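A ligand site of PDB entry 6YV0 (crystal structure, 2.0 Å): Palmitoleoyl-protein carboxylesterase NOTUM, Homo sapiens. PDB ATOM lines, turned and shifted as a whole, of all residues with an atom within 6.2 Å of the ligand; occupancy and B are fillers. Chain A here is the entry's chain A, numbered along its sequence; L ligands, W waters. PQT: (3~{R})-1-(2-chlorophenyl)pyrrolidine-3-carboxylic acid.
An oxygen (O1) of the ligand is in hydrogen-bond range of the backbone NH (N) of Trp 51.
An oxygen (O1) of the ligand is in hydrogen-bond range of the backbone NH (N) of Ala 156, 3.3 Å away.
NE2 of His 312 is in hydrogen-bond range of O of the ligand (3.4 Å).
The backbone carbonyl oxygen of Trp 51 sits at hydrogen-bond distance from the side-chain hydroxyl of Tyr 105 (2.7 Å).
The backbone carbonyl oxygen of Gly 189 is in hydrogen-bond range of the side-chain hydroxyl of Thr 159 (3.0 Å).
OG of Ser 155 sits at hydrogen-bond distance from OE2 of Glu 313.
N of Ala 265 is in hydrogen-bond range of OD2 of Asp 263, at 3.1 Å.
The backbone NH (N) of Val 110 lies within hydrogen-bond range of the side-chain hydroxyl (OH) of Tyr 105 (2.9 Å).
Merely in contact with the ligand: Thr 159 (3.1 Å), Ser 155 (3.2 Å), Tyr 52 (3.4 Å), Phe 191 (3.4 Å), Ala 265 (3.5 Å), Pro 210 (3.5 Å), Ile 214 (3.6 Å), Phe 242 (3.6 Å) and Val 110 (3.7 Å).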
ATOM      1  N   GLY A  49      -6.849 -14.631  -5.808  1.00  0.00           N
ATOM      2  CA  GLY A  49      -7.315 -15.074  -7.098  1.00  0.00           C
ATOM      3  C   GLY A  49      -8.834 -15.225  -7.146  1.00  0.00           C
ATOM      4  O   GLY A  49      -9.555 -14.881  -6.214  1.00  0.00           O
ATOM      5  N   GLY A  50      -9.303 -15.750  -8.279  1.00  0.00           N
ATOM      6  CA  GLY A  50     -10.716 -16.011  -8.425  1.00  0.00           C
ATOM      7  C   GLY A  50     -11.282 -15.796  -9.817  1.00  0.00           C
ATOM      8  O   GLY A  50     -12.343 -15.181  -9.962  1.00  0.00           O
ATOM      9  N   TRP A  51     -10.581 -16.286 -10.827  1.00  0.00           N
ATOM     10  CA  TRP A  51     -11.047 -16.267 -12.226  1.00  0.00           C
ATOM     11  C   TRP A  51     -11.243 -14.807 -12.659  1.00  0.00           C
ATOM     12  O   TRP A  51     -10.422 -13.949 -12.293  1.00  0.00           O
ATOM     13  CB  TRP A  51     -12.274 -17.146 -12.375  1.00  0.00           C
ATOM     14  CG  TRP A  51     -11.982 -18.611 -12.273  1.00  0.00           C
ATOM     15  CD1 TRP A  51     -11.970 -19.361 -11.140  1.00  0.00           C
ATOM     16  CD2 TRP A  51     -11.667 -19.504 -13.347  1.00  0.00           C
ATOM     17  NE1 TRP A  51     -11.654 -20.668 -11.438  1.00  0.00           N
ATOM     18  CE2 TRP A  51     -11.468 -20.776 -12.790  1.00  0.00           C
ATOM     19  CE3 TRP A  51     -11.520 -19.336 -14.731  1.00  0.00           C
ATOM     20  CZ2 TRP A  51     -11.135 -21.894 -13.557  1.00  0.00           C
ATOM     21  CZ3 TRP A  51     -11.190 -20.446 -15.493  1.00  0.00           C
ATOM     22  CH2 TRP A  51     -11.006 -21.704 -14.907  1.00  0.00           C
ATOM     23  N   TYR A  52     -12.299 -14.504 -13.417  1.00  0.00           N
ATOM     24  CA  TYR A  52     -12.497 -13.185 -14.018  1.00  0.00           C
ATOM     25  C   TYR A  52     -13.847 -13.115 -14.709  1.00  0.00           C
ATOM     26  O   TYR A  52     -14.639 -14.067 -14.641  1.00  0.00           O
ATOM     27  CB  TYR A  52     -11.387 -12.884 -15.026  1.00  0.00           C
ATOM     28  CG  TYR A  52     -11.053 -14.066 -15.921  1.00  0.00           C
ATOM     29  CD1 TYR A  52     -11.941 -14.490 -16.898  1.00  0.00           C
ATOM     30  CD2 TYR A  52      -9.851 -14.747 -15.795  1.00  0.00           C
ATOM     31  CE1 TYR A  52     -11.658 -15.565 -17.716  1.00  0.00           C
ATOM     32  CE2 TYR A  52      -9.560 -15.821 -16.609  1.00  0.00           C
ATOM     33  CZ  TYR A  52     -10.460 -16.224 -17.565  1.00  0.00           C
ATOM     34  OH  TYR A  52     -10.160 -17.297 -18.375  1.00  0.00           O
ATOM     35  N   TYR A 105      -9.340  -9.733  -4.094  1.00  0.00           N
ATOM     36  CA  TYR A 105      -9.516  -9.658  -5.541  1.00  0.00           C
ATOM     37  C   TYR A 105     -10.959  -9.254  -5.821  1.00  0.00           C
ATOM     38  O   TYR A 105     -11.871 -10.074  -5.708  1.00  0.00           O
ATOM     39  CB  TYR A 105      -9.163 -11.004  -6.175  1.00  0.00           C
ATOM     40  CG  TYR A 105      -9.309 -11.105  -7.677  1.00  0.00           C
ATOM     41  CD1 TYR A 105      -8.853 -10.085  -8.518  1.00  0.00           C
ATOM     42  CD2 TYR A 105      -9.857 -12.232  -8.260  1.00  0.00           C
ATOM     43  CE1 TYR A 105      -8.977 -10.195  -9.893  1.00  0.00           C
ATOM     44  CE2 TYR A 105      -9.984 -12.347  -9.628  1.00  0.00           C
ATOM     45  CZ  TYR A 105      -9.548 -11.336 -10.444  1.00  0.00           C
ATOM     46  OH  TYR A 105      -9.675 -11.451 -11.811  1.00  0.00           O
ATOM     47  N   VAL A 110      -7.825 -10.036 -13.560  1.00  0.00           N
ATOM     48  CA  VAL A 110      -6.493 -10.620 -13.387  1.00  0.00           C
ATOM     49  C   VAL A 110      -5.511  -9.522 -12.994  1.00  0.00           C
ATOM     50  O   VAL A 110      -4.328  -9.560 -13.363  1.00  0.00           O
ATOM     51  CB  VAL A 110      -6.035 -11.383 -14.649  1.00  0.00           C
ATOM     52  CG1 VAL A 110      -4.937 -12.383 -14.308  1.00  0.00           C
ATOM     53  CG2 VAL A 110      -7.205 -12.101 -15.296  1.00  0.00           C
ATOM     54  N   SER A 154      -1.953 -16.047  -5.898  1.00  0.00           N
ATOM     55  CA  SER A 154      -2.358 -17.388  -6.285  1.00  0.00           C
ATOM     56  C   SER A 154      -3.412 -17.328  -7.378  1.00  0.00           C
ATOM     57  O   SER A 154      -4.288 -16.464  -7.356  1.00  0.00           O
ATOM     58  CB  SER A 154      -2.905 -18.180  -5.077  1.00  0.00           C
ATOM     59  OG  SER A 154      -1.891 -18.393  -4.111  1.00  0.00           O
ATOM     60  N   SER A 155      -3.298 -18.263  -8.338  1.00  0.00           N
ATOM     61  CA  SER A 155      -4.220 -18.384  -9.465  1.00  0.00           C
ATOM     62  C   SER A 155      -4.217 -17.049 -10.221  1.00  0.00           C
ATOM     63  O   SER A 155      -3.145 -16.636 -10.670  1.00  0.00           O
ATOM     64  CB  SER A 155      -5.591 -18.867  -8.968  1.00  0.00           C
ATOM     65  OG  SER A 155      -6.223 -17.892  -8.152  1.00  0.00           O
ATOM     66  N   ALA A 156      -5.355 -16.369 -10.388  1.00  0.00           N
ATOM     67  CA  ALA A 156      -5.371 -15.098 -11.081  1.00  0.00           C
ATOM     68  C   ALA A 156      -4.473 -14.074 -10.379  1.00  0.00           C
ATOM     69  O   ALA A 156      -3.912 -13.192 -11.036  1.00  0.00           O
ATOM     70  CB  ALA A 156      -6.801 -14.560 -11.194  1.00  0.00           C
ATOM     71  N   GLY A 157      -4.333 -14.191  -9.060  1.00  0.00           N
ATOM     72  CA  GLY A 157      -3.362 -13.368  -8.352  1.00  0.00           C
ATOM     73  C   GLY A 157      -1.930 -13.728  -8.695  1.00  0.00           C
ATOM     74  O   GLY A 157      -1.047 -12.877  -8.660  1.00  0.00           O
ATOM     75  N   THR A 159      -0.933 -14.808 -11.746  1.00  0.00           N
ATOM     76  CA  THR A 159      -0.718 -14.098 -13.000  1.00  0.00           C
ATOM     77  C   THR A 159      -0.645 -12.591 -12.770  1.00  0.00           C
ATOM     78  O   THR A 159       0.097 -11.890 -13.471  1.00  0.00           O
ATOM     79  CB  THR A 159      -1.835 -14.424 -13.994  1.00  0.00           C
ATOM     80  OG1 THR A 159      -2.019 -15.846 -14.057  1.00  0.00           O
ATOM     81  CG2 THR A 159      -1.494 -13.901 -15.388  1.00  0.00           C
ATOM     82  N   SER A 188       0.477 -20.797  -9.070  1.00  0.00           N
ATOM     83  CA  SER A 188      -0.624 -21.330  -9.883  1.00  0.00           C
ATOM     84  C   SER A 188      -1.124 -20.312 -10.912  1.00  0.00           C
ATOM     85  O   SER A 188      -2.295 -20.326 -11.284  1.00  0.00           O
ATOM     86  CB  SER A 188      -1.771 -21.805  -9.002  1.00  0.00           C
ATOM     87  OG  SER A 188      -1.349 -22.841  -8.137  1.00  0.00           O
ATOM     88  N   GLY A 189      -0.243 -19.432 -11.370  1.00  0.00           N
ATOM     89  CA  GLY A 189      -0.603 -18.454 -12.377  1.00  0.00           C
ATOM     90  C   GLY A 189       0.230 -18.574 -13.633  1.00  0.00           C
ATOM     91  O   GLY A 189       0.339 -17.623 -14.418  1.00  0.00           O
ATOM     92  N   PHE A 191       0.267 -20.390 -16.907  1.00  0.00           N
ATOM     93  CA  PHE A 191      -0.641 -21.125 -17.759  1.00  0.00           C
ATOM     94  C   PHE A 191      -0.085 -21.268 -19.179  1.00  0.00           C
ATOM     95  O   PHE A 191       0.814 -20.545 -19.597  1.00  0.00           O
ATOM     96  CB  PHE A 191      -2.008 -20.438 -17.815  1.00  0.00           C
ATOM     97  CG  PHE A 191      -2.692 -20.359 -16.483  1.00  0.00           C
ATOM     98  CD1 PHE A 191      -3.352 -21.466 -15.970  1.00  0.00           C
ATOM     99  CD2 PHE A 191      -2.664 -19.192 -15.745  1.00  0.00           C
ATOM    100  CE1 PHE A 191      -3.978 -21.397 -14.737  1.00  0.00           C
ATOM    101  CE2 PHE A 191      -3.287 -19.118 -14.519  1.00  0.00           C
ATOM    102  CZ  PHE A 191      -3.935 -20.219 -14.011  1.00  0.00           C
ATOM    103  N   ALA A 209     -11.460 -21.512 -23.845  1.00  0.00           N
ATOM    104  CA  ALA A 209     -10.025 -21.761 -23.964  1.00  0.00           C
ATOM    105  C   ALA A 209      -9.237 -20.612 -23.356  1.00  0.00           C
ATOM    106  O   ALA A 209      -9.675 -19.464 -23.393  1.00  0.00           O
ATOM    107  CB  ALA A 209      -9.644 -21.937 -25.429  1.00  0.00           C
ATOM    108  N   PRO A 210      -8.050 -20.891 -22.797  1.00  0.00           N
ATOM    109  CA  PRO A 210      -7.304 -19.833 -22.114  1.00  0.00           C
ATOM    110  C   PRO A 210      -6.836 -18.718 -23.038  1.00  0.00           C
ATOM    111  O   PRO A 210      -6.666 -17.579 -22.579  1.00  0.00           O
ATOM    112  CB  PRO A 210      -6.114 -20.582 -21.500  1.00  0.00           C
ATOM    113  CG  PRO A 210      -5.950 -21.793 -22.375  1.00  0.00           C
ATOM    114  CD  PRO A 210      -7.342 -22.179 -22.769  1.00  0.00           C
ATOM    115  N   THR A 211      -6.631 -18.998 -24.321  1.00  0.00           N
ATOM    116  CA  THR A 211      -6.157 -17.959 -25.231  1.00  0.00           C
ATOM    117  C   THR A 211      -7.266 -16.992 -25.610  1.00  0.00           C
ATOM    118  O   THR A 211      -7.052 -15.771 -25.619  1.00  0.00           O
ATOM    119  CB  THR A 211      -5.537 -18.583 -26.482  1.00  0.00           C
ATOM    120  OG1 THR A 211      -5.295 -17.563 -27.461  1.00  0.00           O
ATOM    121  CG2 THR A 211      -6.449 -19.649 -27.066  1.00  0.00           C
ATOM    122  N   ALA A 213     -10.068 -16.414 -23.936  1.00  0.00           N
ATOM    123  CA  ALA A 213     -10.585 -15.708 -22.769  1.00  0.00           C
ATOM    124  C   ALA A 213      -9.814 -14.419 -22.512  1.00  0.00           C
ATOM    125  O   ALA A 213     -10.405 -13.381 -22.201  1.00  0.00           O
ATOM    126  CB  ALA A 213     -10.525 -16.620 -21.539  1.00  0.00           C
ATOM    127  N   ILE A 214      -8.482 -14.476 -22.641  1.00  0.00           N
ATOM    128  CA  ILE A 214      -7.672 -13.290 -22.363  1.00  0.00           C
ATOM    129  C   ILE A 214      -7.793 -12.273 -23.496  1.00  0.00           C
ATOM    130  O   ILE A 214      -7.725 -11.062 -23.251  1.00  0.00           O
ATOM    131  CB  ILE A 214      -6.204 -13.707 -22.132  1.00  0.00           C
ATOM    132  CG1 ILE A 214      -6.107 -14.737 -21.016  1.00  0.00           C
ATOM    133  CG2 ILE A 214      -5.358 -12.490 -21.796  1.00  0.00           C
ATOM    134  CD1 ILE A 214      -6.671 -14.261 -19.693  1.00  0.00           C
ATOM    135  N   PHE A 242      -0.183 -12.344 -20.713  1.00  0.00           N
ATOM    136  CA  PHE A 242      -0.853 -12.990 -19.603  1.00  0.00           C
ATOM    137  C   PHE A 242      -0.372 -14.414 -19.370  1.00  0.00           C
ATOM    138  O   PHE A 242      -0.799 -15.043 -18.387  1.00  0.00           O
ATOM    139  CB  PHE A 242      -2.362 -12.989 -19.822  1.00  0.00           C
ATOM    140  CG  PHE A 242      -3.048 -11.719 -19.429  1.00  0.00           C
ATOM    141  CD1 PHE A 242      -2.780 -10.537 -20.105  1.00  0.00           C
ATOM    142  CD2 PHE A 242      -3.966 -11.698 -18.392  1.00  0.00           C
ATOM    143  CE1 PHE A 242      -3.411  -9.357 -19.752  1.00  0.00           C
ATOM    144  CE2 PHE A 242      -4.600 -10.523 -18.031  1.00  0.00           C
ATOM    145  CZ  PHE A 242      -4.320  -9.348 -18.707  1.00  0.00           C
ATOM    146  N   PHE A 243       0.490 -14.940 -20.235  1.00  0.00           N
ATOM    147  CA  PHE A 243       0.975 -16.309 -20.127  1.00  0.00           C
ATOM    148  C   PHE A 243       2.416 -16.266 -19.653  1.00  0.00           C
ATOM    149  O   PHE A 243       3.263 -15.614 -20.274  1.00  0.00           O
ATOM    150  CB  PHE A 243       0.825 -17.037 -21.456  1.00  0.00           C
ATOM    151  CG  PHE A 243      -0.604 -17.289 -21.838  1.00  0.00           C
ATOM    152  CD1 PHE A 243      -1.244 -18.458 -21.446  1.00  0.00           C
ATOM    153  CD2 PHE A 243      -1.327 -16.346 -22.546  1.00  0.00           C
ATOM    154  CE1 PHE A 243      -2.559 -18.684 -21.771  1.00  0.00           C
ATOM    155  CE2 PHE A 243      -2.639 -16.566 -22.878  1.00  0.00           C
ATOM    156  CZ  PHE A 243      -3.264 -17.737 -22.495  1.00  0.00           C
ATOM    157  N   ASP A 263      -2.198 -28.383 -13.146  1.00  0.00           N
ATOM    158  CA  ASP A 263      -3.073 -27.473 -12.433  1.00  0.00           C
ATOM    159  C   ASP A 263      -4.526 -27.711 -12.839  1.00  0.00           C
ATOM    160  O   ASP A 263      -4.841 -27.791 -14.025  1.00  0.00           O
ATOM    161  CB  ASP A 263      -2.671 -26.026 -12.713  1.00  0.00           C
ATOM    162  CG  ASP A 263      -3.418 -25.040 -11.843  1.00  0.00           C
ATOM    163  OD1 ASP A 263      -3.072 -24.906 -10.648  1.00  0.00           O
ATOM    164  OD2 ASP A 263      -4.366 -24.400 -12.343  1.00  0.00           O
ATOM    165  N   ALA A 265      -7.098 -25.797 -12.763  1.00  0.00           N
ATOM    166  CA  ALA A 265      -7.662 -24.728 -13.570  1.00  0.00           C
ATOM    167  C   ALA A 265      -7.169 -24.823 -15.016  1.00  0.00           C
ATOM    168  O   ALA A 265      -7.920 -24.535 -15.952  1.00  0.00           O
ATOM    169  CB  ALA A 265      -7.324 -23.370 -12.970  1.00  0.00           C
ATOM    170  N   GLN A 266      -5.902 -25.206 -15.209  1.00  0.00           N
ATOM    171  CA  GLN A 266      -5.409 -25.462 -16.550  1.00  0.00           C
ATOM    172  C   GLN A 266      -6.173 -26.610 -17.211  1.00  0.00           C
ATOM    173  O   GLN A 266      -6.553 -26.520 -18.383  1.00  0.00           O
ATOM    174  CB  GLN A 266      -3.914 -25.769 -16.512  1.00  0.00           C
ATOM    175  CG  GLN A 266      -3.309 -26.142 -17.865  1.00  0.00           C
ATOM    176  CD  GLN A 266      -3.006 -24.934 -18.724  1.00  0.00           C
ATOM    177  OE1 GLN A 266      -2.277 -24.025 -18.319  1.00  0.00           O
ATOM    178  NE2 GLN A 266      -3.572 -24.911 -19.930  1.00  0.00           N
ATOM    179  N   VAL A 269      -9.849 -25.253 -18.226  1.00  0.00           N
ATOM    180  CA  VAL A 269      -9.927 -24.515 -19.477  1.00  0.00           C
ATOM    181  C   VAL A 269      -9.523 -25.363 -20.665  1.00  0.00           C
ATOM    182  O   VAL A 269      -9.821 -25.015 -21.813  1.00  0.00           O
ATOM    183  CB  VAL A 269      -9.060 -23.236 -19.405  1.00  0.00           C
ATOM    184  CG1 VAL A 269      -9.585 -22.297 -18.325  1.00  0.00           C
ATOM    185  CG2 VAL A 269      -7.603 -23.588 -19.148  1.00  0.00           C
ATOM    186  N   HIS A 312      -4.545 -27.284  -7.104  1.00  0.00           N
ATOM    187  CA  HIS A 312      -4.793 -25.890  -7.449  1.00  0.00           C
ATOM    188  C   HIS A 312      -4.444 -25.020  -6.243  1.00  0.00           C
ATOM    189  O   HIS A 312      -5.023 -25.205  -5.172  1.00  0.00           O
ATOM    190  CB  HIS A 312      -6.246 -25.683  -7.862  1.00  0.00           C
ATOM    191  CG  HIS A 312      -6.548 -24.307  -8.374  1.00  0.00           C
ATOM    192  ND1 HIS A 312      -7.502 -23.487  -7.798  1.00  0.00           N
ATOM    193  CD2 HIS A 312      -6.012 -23.612  -9.401  1.00  0.00           C
ATOM    194  CE1 HIS A 312      -7.547 -22.340  -8.458  1.00  0.00           C
ATOM    195  NE2 HIS A 312      -6.652 -22.390  -9.435  1.00  0.00           N
ATOM    196  N   GLU A 313      -3.515 -24.081  -6.435  1.00  0.00           N
ATOM    197  CA  GLU A 313      -3.017 -23.171  -5.400  1.00  0.00           C
ATOM    198  C   GLU A 313      -2.284 -23.912  -4.294  1.00  0.00           C
ATOM    199  O   GLU A 313      -2.428 -25.130  -4.147  1.00  0.00           O
ATOM    200  CB  GLU A 313      -4.167 -22.340  -4.811  1.00  0.00           C
ATOM    201  CG  GLU A 313      -4.777 -21.361  -5.780  1.00  0.00           C
ATOM    202  CD  GLU A 313      -5.903 -20.558  -5.163  1.00  0.00           C
ATOM    203  OE1 GLU A 313      -6.415 -20.955  -4.095  1.00  0.00           O
ATOM    204  OE2 GLU A 313      -6.281 -19.528  -5.755  1.00  0.00           O
HETATM  205  C1  PQT L   1      -5.491 -16.510 -15.367  1.00  0.00           C
HETATM  206  C2  PQT L   1      -6.127 -17.455 -16.161  1.00  0.00           C
HETATM  207  C3  PQT L   1      -5.735 -17.574 -17.497  1.00  0.00           C
HETATM  208  C4  PQT L   1      -4.733 -16.781 -18.020  1.00  0.00           C
HETATM  209  C5  PQT L   1      -4.115 -15.853 -17.206  1.00  0.00           C
HETATM  210  C6  PQT L   1      -7.940 -17.859 -14.471  1.00  0.00           C
HETATM  211  C8  PQT L   1      -7.296 -20.153 -14.253  1.00  0.00           C
HETATM  212  C9  PQT L   1      -7.135 -19.732 -15.703  1.00  0.00           C
HETATM  213  C10 PQT L   1      -7.852 -18.906 -12.134  1.00  0.00           C
HETATM  214  O1  PQT L   1      -8.092 -17.699 -11.701  1.00  0.00           O
HETATM  215  N   PQT L   1      -7.158 -18.272 -15.639  1.00  0.00           N
HETATM  216  C   PQT L   1      -4.493 -15.708 -15.885  1.00  0.00           C
HETATM  217  O   PQT L   1      -7.398 -19.808 -11.457  1.00  0.00           O
HETATM  218  C7  PQT L   1      -8.200 -19.092 -13.601  1.00  0.00           C
HETATM  219 CL   PQT L   1      -6.541 -18.680 -18.570  1.00  0.00          CL
HETATM  220  O   HOH W   1      -9.197 -19.815  -8.591  1.00  0.00           O
